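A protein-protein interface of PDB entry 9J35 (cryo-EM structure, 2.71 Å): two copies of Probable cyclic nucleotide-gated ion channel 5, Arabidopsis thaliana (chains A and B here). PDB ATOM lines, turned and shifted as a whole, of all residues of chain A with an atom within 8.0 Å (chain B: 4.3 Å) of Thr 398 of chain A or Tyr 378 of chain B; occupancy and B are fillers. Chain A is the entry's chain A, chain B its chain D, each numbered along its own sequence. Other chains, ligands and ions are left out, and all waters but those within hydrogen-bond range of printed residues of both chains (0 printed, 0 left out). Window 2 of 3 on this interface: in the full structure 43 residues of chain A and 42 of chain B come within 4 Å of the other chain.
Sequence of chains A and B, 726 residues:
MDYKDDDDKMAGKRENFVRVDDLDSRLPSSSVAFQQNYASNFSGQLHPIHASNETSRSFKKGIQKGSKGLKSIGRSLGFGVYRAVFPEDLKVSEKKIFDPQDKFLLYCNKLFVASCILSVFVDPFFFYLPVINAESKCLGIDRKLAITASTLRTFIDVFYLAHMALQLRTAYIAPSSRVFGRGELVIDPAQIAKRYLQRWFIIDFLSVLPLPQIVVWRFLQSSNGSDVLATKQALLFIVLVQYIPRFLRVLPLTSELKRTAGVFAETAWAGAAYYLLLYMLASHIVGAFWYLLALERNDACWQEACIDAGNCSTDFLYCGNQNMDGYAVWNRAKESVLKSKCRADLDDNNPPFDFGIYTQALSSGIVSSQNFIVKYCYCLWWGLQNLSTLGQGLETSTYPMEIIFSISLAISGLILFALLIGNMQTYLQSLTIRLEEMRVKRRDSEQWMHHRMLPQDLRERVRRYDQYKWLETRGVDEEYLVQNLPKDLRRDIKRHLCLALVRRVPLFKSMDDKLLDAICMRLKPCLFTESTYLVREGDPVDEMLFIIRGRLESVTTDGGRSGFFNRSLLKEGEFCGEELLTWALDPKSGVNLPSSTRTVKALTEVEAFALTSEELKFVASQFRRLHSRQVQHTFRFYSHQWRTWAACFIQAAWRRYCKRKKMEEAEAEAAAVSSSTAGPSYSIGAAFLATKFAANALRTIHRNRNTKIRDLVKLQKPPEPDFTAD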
ATOM      1  N   ARG A 297      21.775 -19.962  -5.894  1.00  0.00           N
ATOM      2  CA  ARG A 297      20.971 -20.934  -5.148  1.00  0.00           C
ATOM      3  C   ARG A 297      21.685 -21.445  -3.900  1.00  0.00           C
ATOM      4  O   ARG A 297      21.034 -21.673  -2.871  1.00  0.00           O
ATOM      5  CB  ARG A 297      20.565 -22.118  -6.019  1.00  0.00           C
ATOM      6  CG  ARG A 297      19.616 -21.779  -7.117  1.00  0.00           C
ATOM      7  CD  ARG A 297      18.378 -21.043  -6.644  1.00  0.00           C
ATOM      8  NE  ARG A 297      17.347 -21.901  -6.086  1.00  0.00           N
ATOM      9  CZ  ARG A 297      16.364 -21.456  -5.315  1.00  0.00           C
ATOM     10  NH1 ARG A 297      16.288 -20.173  -5.020  1.00  0.00           N
ATOM     11  NH2 ARG A 297      15.451 -22.286  -4.846  1.00  0.00           N
ATOM     12  N   ASP A 354      16.258 -28.481  -2.668  1.00  0.00           N
ATOM     13  CA  ASP A 354      16.323 -28.902  -4.058  1.00  0.00           C
ATOM     14  C   ASP A 354      17.167 -27.901  -4.835  1.00  0.00           C
ATOM     15  O   ASP A 354      16.905 -26.697  -4.793  1.00  0.00           O
ATOM     16  CB  ASP A 354      14.928 -29.026  -4.664  1.00  0.00           C
ATOM     17  CG  ASP A 354      14.866 -30.050  -5.775  1.00  0.00           C
ATOM     18  OD1 ASP A 354      15.790 -30.866  -5.887  1.00  0.00           O
ATOM     19  OD2 ASP A 354      13.897 -30.051  -6.548  1.00  0.00           O
ATOM     20  N   GLY A 356      18.161 -28.636  -8.298  1.00  0.00           N
ATOM     21  CA  GLY A 356      17.618 -28.631  -9.649  1.00  0.00           C
ATOM     22  C   GLY A 356      18.683 -28.887 -10.697  1.00  0.00           C
ATOM     23  O   GLY A 356      19.314 -29.898 -10.677  1.00  0.00           O
ATOM     24  N   GLU A 395      16.717 -31.677 -15.428  1.00  0.00           N
ATOM     25  CA  GLU A 395      15.698 -32.030 -14.441  1.00  0.00           C
ATOM     26  C   GLU A 395      15.565 -30.878 -13.459  1.00  0.00           C
ATOM     27  O   GLU A 395      16.324 -30.799 -12.497  1.00  0.00           O
ATOM     28  CB  GLU A 395      16.055 -33.321 -13.724  1.00  0.00           C
ATOM     29  CG  GLU A 395      16.317 -34.464 -14.652  1.00  0.00           C
ATOM     30  CD  GLU A 395      16.491 -35.766 -13.937  1.00  0.00           C
ATOM     31  OE1 GLU A 395      17.133 -35.778 -12.869  1.00  0.00           O
ATOM     32  OE2 GLU A 395      15.985 -36.789 -14.442  1.00  0.00           O
ATOM     33  N   THR A 396      14.586 -30.009 -13.687  1.00  0.00           N
ATOM     34  CA  THR A 396      14.418 -28.795 -12.912  1.00  0.00           C
ATOM     35  C   THR A 396      13.764 -29.078 -11.564  1.00  0.00           C
ATOM     36  O   THR A 396      13.361 -30.191 -11.247  1.00  0.00           O
ATOM     37  CB  THR A 396      13.558 -27.778 -13.662  1.00  0.00           C
ATOM     38  OG1 THR A 396      12.260 -28.328 -13.872  1.00  0.00           O
ATOM     39  CG2 THR A 396      14.154 -27.410 -14.988  1.00  0.00           C
ATOM     40  N   SER A 397      13.682 -28.036 -10.766  1.00  0.00           N
ATOM     41  CA  SER A 397      12.831 -27.971  -9.598  1.00  0.00           C
ATOM     42  C   SER A 397      11.602 -27.133  -9.941  1.00  0.00           C
ATOM     43  O   SER A 397      11.399 -26.732 -11.085  1.00  0.00           O
ATOM     44  CB  SER A 397      13.616 -27.409  -8.418  1.00  0.00           C
ATOM     45  OG  SER A 397      13.893 -26.041  -8.575  1.00  0.00           O
ATOM     46  N   THR A 398      10.779 -26.840  -8.944  1.00  0.00           N
ATOM     47  CA  THR A 398       9.579 -26.043  -9.137  1.00  0.00           C
ATOM     48  C   THR A 398       9.826 -24.560  -8.904  1.00  0.00           C
ATOM     49  O   THR A 398       8.898 -23.828  -8.573  1.00  0.00           O
ATOM     50  CB  THR A 398       8.456 -26.538  -8.228  1.00  0.00           C
ATOM     51  OG1 THR A 398       8.796 -26.285  -6.865  1.00  0.00           O
ATOM     52  CG2 THR A 398       8.218 -28.018  -8.410  1.00  0.00           C
ATOM     53  N   TYR A 399      11.061 -24.104  -9.072  1.00  0.00           N
ATOM     54  CA  TYR A 399      11.409 -22.703  -8.902  1.00  0.00           C
ATOM     55  C   TYR A 399      11.268 -22.004 -10.249  1.00  0.00           C
ATOM     56  O   TYR A 399      11.875 -22.454 -11.225  1.00  0.00           O
ATOM     57  CB  TYR A 399      12.824 -22.587  -8.364  1.00  0.00           C
ATOM     58  CG  TYR A 399      13.282 -21.181  -8.110  1.00  0.00           C
ATOM     59  CD1 TYR A 399      14.439 -20.690  -8.697  1.00  0.00           C
ATOM     60  CD2 TYR A 399      12.568 -20.343  -7.274  1.00  0.00           C
ATOM     61  CE1 TYR A 399      14.860 -19.405  -8.471  1.00  0.00           C
ATOM     62  CE2 TYR A 399      12.978 -19.050  -7.044  1.00  0.00           C
ATOM     63  CZ  TYR A 399      14.127 -18.591  -7.641  1.00  0.00           C
ATOM     64  OH  TYR A 399      14.540 -17.308  -7.408  1.00  0.00           O
ATOM     65  N   PRO A 400      10.484 -20.924 -10.356  1.00  0.00           N
ATOM     66  CA  PRO A 400      10.052 -20.450 -11.683  1.00  0.00           C
ATOM     67  C   PRO A 400      11.104 -19.781 -12.555  1.00  0.00           C
ATOM     68  O   PRO A 400      10.903 -19.738 -13.770  1.00  0.00           O
ATOM     69  CB  PRO A 400       8.927 -19.467 -11.337  1.00  0.00           C
ATOM     70  CG  PRO A 400       8.416 -19.913 -10.074  1.00  0.00           C
ATOM     71  CD  PRO A 400       9.584 -20.427  -9.306  1.00  0.00           C
ATOM     72  N   MET A 401      12.188 -19.228 -12.013  1.00  0.00           N
ATOM     73  CA  MET A 401      13.204 -18.624 -12.869  1.00  0.00           C
ATOM     74  C   MET A 401      14.156 -19.650 -13.461  1.00  0.00           C
ATOM     75  O   MET A 401      14.667 -19.448 -14.573  1.00  0.00           O
ATOM     76  CB  MET A 401      14.000 -17.576 -12.095  1.00  0.00           C
ATOM     77  CG  MET A 401      13.165 -16.462 -11.500  1.00  0.00           C
ATOM     78  SD  MET A 401      12.150 -15.510 -12.658  1.00  0.00           S
ATOM     79  CE  MET A 401      13.381 -14.823 -13.758  1.00  0.00           C
ATOM     80  N   GLU A 402      14.368 -20.753 -12.747  1.00  0.00           N
ATOM     81  CA  GLU A 402      15.054 -21.919 -13.277  1.00  0.00           C
ATOM     82  C   GLU A 402      14.346 -22.513 -14.496  1.00  0.00           C
ATOM     83  O   GLU A 402      15.008 -23.033 -15.395  1.00  0.00           O
ATOM     84  CB  GLU A 402      15.186 -22.938 -12.153  1.00  0.00           C
ATOM     85  CG  GLU A 402      15.914 -24.190 -12.495  1.00  0.00           C
ATOM     86  CD  GLU A 402      16.055 -25.093 -11.327  1.00  0.00           C
ATOM     87  OE1 GLU A 402      16.000 -24.608 -10.194  1.00  0.00           O
ATOM     88  OE2 GLU A 402      16.209 -26.299 -11.529  1.00  0.00           O
ATOM     89  N   ILE A 403      13.014 -22.427 -14.548  1.00  0.00           N
ATOM     90  CA  ILE A 403      12.218 -22.972 -15.642  1.00  0.00           C
ATOM     91  C   ILE A 403      12.297 -22.084 -16.881  1.00  0.00           C
ATOM     92  O   ILE A 403      12.417 -22.583 -18.008  1.00  0.00           O
ATOM     93  CB  ILE A 403      10.772 -23.183 -15.135  1.00  0.00           C
ATOM     94  CG1 ILE A 403      10.682 -24.439 -14.273  1.00  0.00           C
ATOM     95  CG2 ILE A 403       9.763 -23.287 -16.253  1.00  0.00           C
ATOM     96  CD1 ILE A 403       9.477 -24.513 -13.419  1.00  0.00           C
ATOM     97  N   ILE A 407      13.650 -22.974 -20.766  1.00  0.00           N
ATOM     98  CA  ILE A 407      12.868 -22.671 -21.969  1.00  0.00           C
ATOM     99  C   ILE A 407      13.696 -21.871 -22.974  1.00  0.00           C
ATOM    100  O   ILE A 407      13.677 -22.150 -24.184  1.00  0.00           O
ATOM    101  CB  ILE A 407      11.560 -21.951 -21.569  1.00  0.00           C
ATOM    102  CG1 ILE A 407      10.651 -22.897 -20.794  1.00  0.00           C
ATOM    103  CG2 ILE A 407      10.792 -21.432 -22.759  1.00  0.00           C
ATOM    104  CD1 ILE A 407       9.460 -22.254 -20.183  1.00  0.00           C
ATOM    105  N   GLN B 360       5.649 -37.956 -12.189  1.00  0.00           N
ATOM    106  CA  GLN B 360       6.357 -36.698 -11.991  1.00  0.00           C
ATOM    107  C   GLN B 360       5.437 -35.578 -11.529  1.00  0.00           C
ATOM    108  O   GLN B 360       5.901 -34.623 -10.917  1.00  0.00           O
ATOM    109  CB  GLN B 360       7.045 -36.310 -13.298  1.00  0.00           C
ATOM    110  CG  GLN B 360       8.154 -35.310 -13.193  1.00  0.00           C
ATOM    111  CD  GLN B 360       8.651 -34.887 -14.543  1.00  0.00           C
ATOM    112  OE1 GLN B 360       8.881 -35.715 -15.408  1.00  0.00           O
ATOM    113  NE2 GLN B 360       8.802 -33.594 -14.741  1.00  0.00           N
ATOM    114  N   SER B 364       5.974 -34.441  -7.272  1.00  0.00           N
ATOM    115  CA  SER B 364       6.451 -33.091  -7.013  1.00  0.00           C
ATOM    116  C   SER B 364       5.446 -32.247  -6.248  1.00  0.00           C
ATOM    117  O   SER B 364       5.843 -31.285  -5.592  1.00  0.00           O
ATOM    118  CB  SER B 364       6.802 -32.397  -8.321  1.00  0.00           C
ATOM    119  OG  SER B 364       5.678 -32.274  -9.152  1.00  0.00           O
ATOM    120  N   ILE B 366       2.554 -30.587  -7.554  1.00  0.00           N
ATOM    121  CA  ILE B 366       1.888 -29.481  -8.234  1.00  0.00           C
ATOM    122  C   ILE B 366       0.382 -29.671  -8.330  1.00  0.00           C
ATOM    123  O   ILE B 366      -0.331 -28.716  -8.659  1.00  0.00           O
ATOM    124  CB  ILE B 366       2.434 -29.232  -9.655  1.00  0.00           C
ATOM    125  CG1 ILE B 366       2.305 -30.483 -10.525  1.00  0.00           C
ATOM    126  CG2 ILE B 366       3.845 -28.638  -9.610  1.00  0.00           C
ATOM    127  CD1 ILE B 366       2.440 -30.228 -11.972  1.00  0.00           C
ATOM    128  N   VAL B 374       3.600 -21.356 -10.470  1.00  0.00           N
ATOM    129  CA  VAL B 374       4.412 -22.562 -10.365  1.00  0.00           C
ATOM    130  C   VAL B 374       3.784 -23.708 -11.147  1.00  0.00           C
ATOM    131  O   VAL B 374       4.456 -24.392 -11.934  1.00  0.00           O
ATOM    132  CB  VAL B 374       4.581 -22.907  -8.872  1.00  0.00           C
ATOM    133  CG1 VAL B 374       5.226 -24.255  -8.678  1.00  0.00           C
ATOM    134  CG2 VAL B 374       5.359 -21.833  -8.174  1.00  0.00           C
ATOM    135  N   LYS B 375       2.477 -23.889 -10.982  1.00  0.00           N
ATOM    136  CA  LYS B 375       1.715 -24.949 -11.618  1.00  0.00           C
ATOM    137  C   LYS B 375       1.662 -24.786 -13.129  1.00  0.00           C
ATOM    138  O   LYS B 375       1.786 -25.770 -13.860  1.00  0.00           O
ATOM    139  CB  LYS B 375       0.309 -24.961 -11.024  1.00  0.00           C
ATOM    140  CG  LYS B 375      -0.558 -26.085 -11.479  1.00  0.00           C
ATOM    141  CD  LYS B 375      -1.984 -25.711 -11.351  1.00  0.00           C
ATOM    142  CE  LYS B 375      -2.520 -26.110 -10.009  1.00  0.00           C
ATOM    143  NZ  LYS B 375      -3.970 -26.334 -10.093  1.00  0.00           N
ATOM    144  N   TYR B 376       1.495 -23.553 -13.606  1.00  0.00           N
ATOM    145  CA  TYR B 376       1.452 -23.292 -15.037  1.00  0.00           C
ATOM    146  C   TYR B 376       2.808 -23.534 -15.691  1.00  0.00           C
ATOM    147  O   TYR B 376       2.896 -24.207 -16.730  1.00  0.00           O
ATOM    148  CB  TYR B 376       0.984 -21.859 -15.284  1.00  0.00           C
ATOM    149  CG  TYR B 376       0.951 -21.517 -16.742  1.00  0.00           C
ATOM    150  CD1 TYR B 376       1.937 -20.729 -17.319  1.00  0.00           C
ATOM    151  CD2 TYR B 376      -0.043 -22.012 -17.555  1.00  0.00           C
ATOM    152  CE1 TYR B 376       1.923 -20.451 -18.647  1.00  0.00           C
ATOM    153  CE2 TYR B 376      -0.057 -21.738 -18.888  1.00  0.00           C
ATOM    154  CZ  TYR B 376       0.926 -20.957 -19.426  1.00  0.00           C
ATOM    155  OH  TYR B 376       0.907 -20.681 -20.759  1.00  0.00           O
ATOM    156  N   CYS B 377       3.876 -22.971 -15.103  1.00  0.00           N
ATOM    157  CA  CYS B 377       5.208 -23.017 -15.697  1.00  0.00           C
ATOM    158  C   CYS B 377       5.769 -24.429 -15.735  1.00  0.00           C
ATOM    159  O   CYS B 377       6.389 -24.818 -16.736  1.00  0.00           O
ATOM    160  CB  CYS B 377       6.149 -22.110 -14.913  1.00  0.00           C
ATOM    161  SG  CYS B 377       5.936 -20.354 -15.153  1.00  0.00           S
ATOM    162  N   TYR B 378       5.531 -25.208 -14.673  1.00  0.00           N
ATOM    163  CA  TYR B 378       5.973 -26.594 -14.614  1.00  0.00           C
ATOM    164  C   TYR B 378       5.385 -27.461 -15.726  1.00  0.00           C
ATOM    165  O   TYR B 378       6.094 -28.292 -16.293  1.00  0.00           O
ATOM    166  CB  TYR B 378       5.614 -27.170 -13.249  1.00  0.00           C
ATOM    167  CG  TYR B 378       6.391 -28.397 -12.880  1.00  0.00           C
ATOM    168  CD1 TYR B 378       5.830 -29.655 -13.005  1.00  0.00           C
ATOM    169  CD2 TYR B 378       7.687 -28.300 -12.427  1.00  0.00           C
ATOM    170  CE1 TYR B 378       6.537 -30.781 -12.686  1.00  0.00           C
ATOM    171  CE2 TYR B 378       8.403 -29.422 -12.101  1.00  0.00           C
ATOM    172  CZ  TYR B 378       7.821 -30.657 -12.235  1.00  0.00           C
ATOM    173  OH  TYR B 378       8.521 -31.780 -11.914  1.00  0.00           O
ATOM    174  N   CYS B 379       4.111 -27.281 -16.052  1.00  0.00           N
ATOM    175  CA  CYS B 379       3.415 -28.061 -17.065  1.00  0.00           C
ATOM    176  C   CYS B 379       3.741 -27.623 -18.487  1.00  0.00           C
ATOM    177  O   CYS B 379       3.880 -28.472 -19.376  1.00  0.00           O
ATOM    178  CB  CYS B 379       1.906 -27.975 -16.823  1.00  0.00           C
ATOM    179  SG  CYS B 379       1.333 -28.819 -15.387  1.00  0.00           S
ATOM    180  N   LEU B 380       3.863 -26.316 -18.713  1.00  0.00           N
ATOM    181  CA  LEU B 380       4.266 -25.816 -20.019  1.00  0.00           C
ATOM    182  C   LEU B 380       5.685 -26.240 -20.393  1.00  0.00           C
ATOM    183  O   LEU B 380       5.947 -26.545 -21.566  1.00  0.00           O
ATOM    184  CB  LEU B 380       4.127 -24.295 -20.038  1.00  0.00           C
ATOM    185  CG  LEU B 380       4.748 -23.430 -21.135  1.00  0.00           C
ATOM    186  CD1 LEU B 380       3.903 -23.431 -22.366  1.00  0.00           C
ATOM    187  CD2 LEU B 380       4.938 -22.033 -20.633  1.00  0.00           C
ATOM    188  N   TRP B 381       6.606 -26.297 -19.421  1.00  0.00           N
ATOM    189  CA  TRP B 381       7.936 -26.806 -19.726  1.00  0.00           C
ATOM    190  C   TRP B 381       7.941 -28.322 -19.972  1.00  0.00           C
ATOM    191  O   TRP B 381       8.743 -28.794 -20.781  1.00  0.00           O
ATOM    192  CB  TRP B 381       8.926 -26.383 -18.622  1.00  0.00           C
ATOM    193  CG  TRP B 381      10.279 -27.119 -18.615  1.00  0.00           C
ATOM    194  CD1 TRP B 381      10.748 -27.910 -17.630  1.00  0.00           C
ATOM    195  CD2 TRP B 381      11.290 -27.134 -19.647  1.00  0.00           C
ATOM    196  NE1 TRP B 381      11.966 -28.421 -17.964  1.00  0.00           N
ATOM    197  CE2 TRP B 381      12.320 -27.967 -19.201  1.00  0.00           C
ATOM    198  CE3 TRP B 381      11.407 -26.544 -20.908  1.00  0.00           C
ATOM    199  CZ2 TRP B 381      13.468 -28.201 -19.949  1.00  0.00           C
ATOM    200  CZ3 TRP B 381      12.527 -26.796 -21.650  1.00  0.00           C
ATOM    201  CH2 TRP B 381      13.543 -27.620 -21.173  1.00  0.00           C
ATOM    202  N   TRP B 382       7.051 -29.092 -19.335  1.00  0.00           N
ATOM    203  CA  TRP B 382       6.895 -30.508 -19.676  1.00  0.00           C
ATOM    204  C   TRP B 382       6.451 -30.686 -21.126  1.00  0.00           C
ATOM    205  O   TRP B 382       7.008 -31.517 -21.858  1.00  0.00           O
ATOM    206  CB  TRP B 382       5.901 -31.188 -18.713  1.00  0.00           C
ATOM    207  CG  TRP B 382       5.892 -32.709 -18.799  1.00  0.00           C
ATOM    208  CD1 TRP B 382       6.589 -33.565 -18.035  1.00  0.00           C
ATOM    209  CD2 TRP B 382       5.162 -33.522 -19.734  1.00  0.00           C
ATOM    210  NE1 TRP B 382       6.358 -34.850 -18.417  1.00  0.00           N
ATOM    211  CE2 TRP B 382       5.485 -34.853 -19.464  1.00  0.00           C
ATOM    212  CE3 TRP B 382       4.261 -33.246 -20.768  1.00  0.00           C
ATOM    213  CZ2 TRP B 382       4.951 -35.909 -20.188  1.00  0.00           C
ATOM    214  CZ3 TRP B 382       3.747 -34.276 -21.482  1.00  0.00           C
ATOM    215  CH2 TRP B 382       4.082 -35.600 -21.190  1.00  0.00           C
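The side-chain hydroxyl (OH) of Tyr 378 of chain B is in hydrogen-bond range of the side-chain amide nitrogen (NE2) of Gln 360 of chain B (3.4 Å).
NE1 of Trp 381 of chain B touches CG2 of Thr 396 of chain A, at 3.8 Å. Val 374 of chain B touches Thr 398 of chain A (CG1 to O, 3.7 Å). CE2 of Tyr 378 of chain B touches CG2 of Thr 398 of chain A, 3.95 Å away. Ile 403 of chain A touches Cys 377 of chain B (CG2 to O, 3.7 Å). CB of Trp 381 of chain B touches CG2 of Ile 403 of chain A, at 3.99 Å. Ile 407 of chain A touches Trp 381 of chain B (CG1 to CE3, 3.7 Å).
Of the printed residues of chain B, Thr 396 of chain A touches Trp 381. Printed residues of chain B within 4 Å of Ile 403 of chain A: Cys 377 and Trp 381. Ile 366 of chain B touches none of the printed residues of chain A. Printed residues of chain A within 4 Å of Val 374 of chain B: Thr 398 (3.7 Å). Printed residues of chain A within 4 Å of Cys 377 of chain B: Ile 403 (3.7 Å). Leu 380 of chain B touches none of the printed residues of chain A. Of the printed residues of chain A, Trp 381 of chain B touches Thr 396 (3.8 Å), Ile 403 (3.99 Å) and Ile 407 (3.7 Å). The nearest residue of chain A that does not touch Tyr 378 of chain B is Ser 397 of chain A (4.2 Å).
No position is printed for both chains. Of the 6 pairs that touch across the chains among the printed residues, none has its exchanged pair printed and touching as well.
Printed residues of chain A that touch a printed residue of chain B: Thr 396, Thr 398, Ile 403 and Ile 407. Among the printed residues, 6 pairs touch across the chains. Among the printed residues, no Asp or Glu carboxylate lies within 4 Å of a Lys or Arg side-chain nitrogen of the other chain.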
